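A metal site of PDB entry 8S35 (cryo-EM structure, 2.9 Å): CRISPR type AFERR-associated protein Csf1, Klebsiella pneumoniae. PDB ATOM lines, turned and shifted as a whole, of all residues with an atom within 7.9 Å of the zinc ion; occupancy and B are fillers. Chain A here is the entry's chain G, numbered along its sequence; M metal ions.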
ATOM      1  N   VAL A   5      23.836  19.480  30.644  1.00  0.00           N
ATOM      2  CA  VAL A   5      22.632  19.985  30.005  1.00  0.00           C
ATOM      3  C   VAL A   5      22.696  19.782  28.498  1.00  0.00           C
ATOM      4  O   VAL A   5      21.666  19.571  27.842  1.00  0.00           O
ATOM      5  CB  VAL A   5      22.403  21.475  30.337  1.00  0.00           C
ATOM      6  CG1 VAL A   5      21.001  21.903  29.903  1.00  0.00           C
ATOM      7  CG2 VAL A   5      22.565  21.739  31.832  1.00  0.00           C
ATOM      8  N   GLU A   6      23.896  19.815  27.909  1.00  0.00           N
ATOM      9  CA  GLU A   6      24.019  19.664  26.467  1.00  0.00           C
ATOM     10  C   GLU A   6      23.551  18.296  26.010  1.00  0.00           C
ATOM     11  O   GLU A   6      22.865  18.172  24.978  1.00  0.00           O
ATOM     12  CB  GLU A   6      25.484  19.879  26.047  1.00  0.00           C
ATOM     13  CG  GLU A   6      25.910  21.335  25.952  1.00  0.00           C
ATOM     14  CD  GLU A   6      26.030  22.016  27.300  1.00  0.00           C
ATOM     15  OE1 GLU A   6      25.395  21.534  28.269  1.00  0.00           O
ATOM     16  OE2 GLU A   6      26.763  23.019  27.400  1.00  0.00           O
ATOM     17  N   ASN A  29      27.735  34.923  31.571  1.00  0.00           N
ATOM     18  CA  ASN A  29      27.507  33.494  31.723  1.00  0.00           C
ATOM     19  C   ASN A  29      26.025  33.181  31.813  1.00  0.00           C
ATOM     20  O   ASN A  29      25.222  33.991  32.300  1.00  0.00           O
ATOM     21  CB  ASN A  29      28.231  32.971  32.972  1.00  0.00           C
ATOM     22  CG  ASN A  29      27.878  33.754  34.220  1.00  0.00           C
ATOM     23  OD1 ASN A  29      27.032  34.654  34.188  1.00  0.00           O
ATOM     24  ND2 ASN A  29      28.514  33.411  35.332  1.00  0.00           N
ATOM     25  N   CYS A  30      25.645  31.999  31.329  1.00  0.00           N
ATOM     26  CA  CYS A  30      24.252  31.570  31.362  1.00  0.00           C
ATOM     27  C   CYS A  30      23.782  31.453  32.804  1.00  0.00           C
ATOM     28  O   CYS A  30      24.251  30.580  33.538  1.00  0.00           O
ATOM     29  CB  CYS A  30      24.054  30.248  30.635  1.00  0.00           C
ATOM     30  SG  CYS A  30      22.498  29.431  31.016  1.00  0.00           S
ATOM     31  N   SER A  31      22.857  32.321  33.204  1.00  0.00           N
ATOM     32  CA  SER A  31      22.372  32.303  34.574  1.00  0.00           C
ATOM     33  C   SER A  31      21.720  30.982  34.949  1.00  0.00           C
ATOM     34  O   SER A  31      21.670  30.632  36.130  1.00  0.00           O
ATOM     35  CB  SER A  31      21.369  33.445  34.784  1.00  0.00           C
ATOM     36  OG  SER A  31      20.541  33.194  35.913  1.00  0.00           O
ATOM     37  N   CYS A  32      21.219  30.229  33.966  1.00  0.00           N
ATOM     38  CA  CYS A  32      20.467  29.022  34.273  1.00  0.00           C
ATOM     39  C   CYS A  32      21.403  27.882  34.658  1.00  0.00           C
ATOM     40  O   CYS A  32      21.278  27.319  35.756  1.00  0.00           O
ATOM     41  CB  CYS A  32      19.565  28.657  33.089  1.00  0.00           C
ATOM     42  SG  CYS A  32      19.120  26.928  32.947  1.00  0.00           S
ATOM     43  N   CYS A  33      22.358  27.531  33.789  1.00  0.00           N
ATOM     44  CA  CYS A  33      23.323  26.485  34.161  1.00  0.00           C
ATOM     45  C   CYS A  33      24.520  27.054  34.910  1.00  0.00           C
ATOM     46  O   CYS A  33      25.057  26.386  35.809  1.00  0.00           O
ATOM     47  CB  CYS A  33      23.824  25.720  32.928  1.00  0.00           C
ATOM     48  SG  CYS A  33      24.572  26.737  31.657  1.00  0.00           S
ATOM     49  N   GLY A  34      24.953  28.267  34.572  1.00  0.00           N
ATOM     50  CA  GLY A  34      26.016  28.927  35.278  1.00  0.00           C
ATOM     51  C   GLY A  34      27.410  28.771  34.700  1.00  0.00           C
ATOM     52  O   GLY A  34      28.337  29.428  35.182  1.00  0.00           O
ATOM     53  N   ARG A  35      27.586  27.948  33.672  1.00  0.00           N
ATOM     54  CA  ARG A  35      28.924  27.778  33.125  1.00  0.00           C
ATOM     55  C   ARG A  35      29.319  29.027  32.324  1.00  0.00           C
ATOM     56  O   ARG A  35      28.507  29.915  32.063  1.00  0.00           O
ATOM     57  CB  ARG A  35      29.002  26.526  32.243  1.00  0.00           C
ATOM     58  CG  ARG A  35      28.235  26.612  30.942  1.00  0.00           C
ATOM     59  CD  ARG A  35      28.259  25.286  30.220  1.00  0.00           C
ATOM     60  NE  ARG A  35      27.404  24.289  30.848  1.00  0.00           N
ATOM     61  CZ  ARG A  35      26.184  23.940  30.440  1.00  0.00           C
ATOM     62  NH1 ARG A  35      25.597  24.539  29.411  1.00  0.00           N
ATOM     63  NH2 ARG A  35      25.531  22.978  31.085  1.00  0.00           N
ATOM     64  N   PHE A  40      29.851  28.490  25.051  1.00  0.00           N
ATOM     65  CA  PHE A  40      28.662  28.794  24.258  1.00  0.00           C
ATOM     66  C   PHE A  40      29.000  29.290  22.856  1.00  0.00           C
ATOM     67  O   PHE A  40      28.079  29.572  22.082  1.00  0.00           O
ATOM     68  CB  PHE A  40      27.791  29.832  24.974  1.00  0.00           C
ATOM     69  CG  PHE A  40      27.334  29.411  26.347  1.00  0.00           C
ATOM     70  CD1 PHE A  40      27.241  28.063  26.697  1.00  0.00           C
ATOM     71  CD2 PHE A  40      26.983  30.359  27.282  1.00  0.00           C
ATOM     72  CE1 PHE A  40      26.822  27.697  27.954  1.00  0.00           C
ATOM     73  CE2 PHE A  40      26.564  29.993  28.539  1.00  0.00           C
ATOM     74  CZ  PHE A  40      26.478  28.658  28.873  1.00  0.00           C
ATOM     75  N   VAL A  56      20.187  35.117  30.743  1.00  0.00           N
ATOM     76  CA  VAL A  56      20.707  34.533  29.523  1.00  0.00           C
ATOM     77  C   VAL A  56      20.670  33.011  29.672  1.00  0.00           C
ATOM     78  O   VAL A  56      21.147  32.466  30.672  1.00  0.00           O
ATOM     79  CB  VAL A  56      22.137  35.021  29.221  1.00  0.00           C
ATOM     80  CG1 VAL A  56      22.091  36.429  28.647  1.00  0.00           C
ATOM     81  CG2 VAL A  56      23.028  34.983  30.459  1.00  0.00           C
ATOM     82  N   HIS A  57      20.099  32.347  28.681  1.00  0.00           N
ATOM     83  CA  HIS A  57      20.025  30.895  28.625  1.00  0.00           C
ATOM     84  C   HIS A  57      20.715  30.424  27.361  1.00  0.00           C
ATOM     85  O   HIS A  57      20.377  30.889  26.266  1.00  0.00           O
ATOM     86  CB  HIS A  57      18.574  30.400  28.645  1.00  0.00           C
ATOM     87  CG  HIS A  57      17.833  30.766  29.890  1.00  0.00           C
ATOM     88  ND1 HIS A  57      18.466  31.141  31.051  1.00  0.00           N
ATOM     89  CD2 HIS A  57      16.510  30.813  30.157  1.00  0.00           C
ATOM     90  CE1 HIS A  57      17.561  31.402  31.986  1.00  0.00           C
ATOM     91  NE2 HIS A  57      16.360  31.211  31.466  1.00  0.00           N
ATOM     92  N   CYS A  58      21.664  29.515  27.494  1.00  0.00           N
ATOM     93  CA  CYS A  58      22.357  29.010  26.333  1.00  0.00           C
ATOM     94  C   CYS A  58      21.427  28.087  25.534  1.00  0.00           C
ATOM     95  O   CYS A  58      20.312  27.788  25.959  1.00  0.00           O
ATOM     96  CB  CYS A  58      23.645  28.279  26.727  1.00  0.00           C
ATOM     97  SG  CYS A  58      23.445  27.067  28.033  1.00  0.00           S
ATOM     98  N   ARG A  59      21.910  27.677  24.369  1.00  0.00           N
ATOM     99  CA  ARG A  59      21.141  26.809  23.468  1.00  0.00           C
ATOM    100  C   ARG A  59      20.504  25.622  24.192  1.00  0.00           C
ATOM    101  O   ARG A  59      19.273  25.464  24.081  1.00  0.00           O
ATOM    102  CB  ARG A  59      22.064  26.345  22.336  1.00  0.00           C
ATOM    103  CG  ARG A  59      21.576  25.129  21.533  1.00  0.00           C
ATOM    104  CD  ARG A  59      20.219  25.367  20.891  1.00  0.00           C
ATOM    105  NE  ARG A  59      20.216  26.516  19.997  1.00  0.00           N
ATOM    106  CZ  ARG A  59      20.810  26.557  18.814  1.00  0.00           C
ATOM    107  NH1 ARG A  59      21.481  25.516  18.338  1.00  0.00           N
ATOM    108  NH2 ARG A  59      20.736  27.664  18.080  1.00  0.00           N
ATOM    109  N   PRO A  60      21.233  24.793  24.934  1.00  0.00           N
ATOM    110  CA  PRO A  60      20.575  23.646  25.582  1.00  0.00           C
ATOM    111  C   PRO A  60      19.735  24.037  26.784  1.00  0.00           C
ATOM    112  O   PRO A  60      18.877  23.245  27.192  1.00  0.00           O
ATOM    113  CB  PRO A  60      21.765  22.764  25.985  1.00  0.00           C
ATOM    114  CG  PRO A  60      22.842  23.739  26.251  1.00  0.00           C
ATOM    115  CD  PRO A  60      22.678  24.810  25.204  1.00  0.00           C
ATOM    116  N   CYS A  61      19.955  25.218  27.360  1.00  0.00           N
ATOM    117  CA  CYS A  61      19.212  25.639  28.540  1.00  0.00           C
ATOM    118  C   CYS A  61      17.923  26.364  28.177  1.00  0.00           C
ATOM    119  O   CYS A  61      16.910  26.197  28.852  1.00  0.00           O
ATOM    120  CB  CYS A  61      20.081  26.565  29.392  1.00  0.00           C
ATOM    121  SG  CYS A  61      21.123  25.680  30.565  1.00  0.00           S
ATOM    122  N   GLN A  62      17.944  27.154  27.098  1.00  0.00           N
ATOM    123  CA  GLN A  62      16.754  27.881  26.696  1.00  0.00           C
ATOM    124  C   GLN A  62      15.609  26.959  26.306  1.00  0.00           C
ATOM    125  O   GLN A  62      14.449  27.372  26.372  1.00  0.00           O
ATOM    126  CB  GLN A  62      17.093  28.817  25.526  1.00  0.00           C
ATOM    127  CG  GLN A  62      15.905  29.525  24.893  1.00  0.00           C
ATOM    128  CD  GLN A  62      15.028  30.231  25.896  1.00  0.00           C
ATOM    129  OE1 GLN A  62      15.488  30.650  26.959  1.00  0.00           O
ATOM    130  NE2 GLN A  62      13.748  30.369  25.578  1.00  0.00           N
ATOM    131  N   VAL A 160      19.001  22.116  36.137  1.00  0.00           N
ATOM    132  CA  VAL A 160      20.189  22.054  35.295  1.00  0.00           C
ATOM    133  C   VAL A 160      21.441  21.960  36.144  1.00  0.00           C
ATOM    134  O   VAL A 160      22.415  21.289  35.771  1.00  0.00           O
ATOM    135  CB  VAL A 160      20.234  23.243  34.307  1.00  0.00           C
ATOM    136  CG1 VAL A 160      19.048  23.189  33.364  1.00  0.00           C
ATOM    137  CG2 VAL A 160      20.288  24.575  35.026  1.00  0.00           C
HETATM  138 ZN    ZN M   1      22.810  27.253  30.259  1.00  0.00          ZN
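NH1 of Arg 35 touches the zinc ion, at 3.98 Å.
Of the 18 residues printed, 5 come within 4 Å of the zinc ion.
Along chain A the residues within 4 Å of the zinc ion span positions 30 to 61.
The nearest printed residue that does not touch the zinc ion is Phe 40 (4.2 Å).
The zinc ion is bound by SG of Cys 33 (2.3 Å), SG of Cys 58 (2.3 Å), SG of Cys 30 (2.3 Å) and SG of Cys 61 (2.3 Å).
The zinc ion has four donor atoms within binding distance.
The guanidinium group of Arg 35 lies close to the side-chain sulfur of Cys 33, 3.3 Å away.
The guanidinium group (NH1) of Arg 35 sits close to the side-chain sulfur (SG) of Cys 58, 3.6 Å away.
The side-chain sulfur (SG) of Cys 30 lies close to the backbone NH (N) of Cys 32, 3.3 Å away.
O of Val 56 lies close to SG of Cys 30, 3.3 Å away.
The side-chain sulfur (SG) of Cys 61 sits close to the side-chain sulfur (SG) of Cys 32 (3.4 Å).
NH1 of Arg 35 is in salt-bridge range of OE2 of Glu 6 (2.8 Å).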
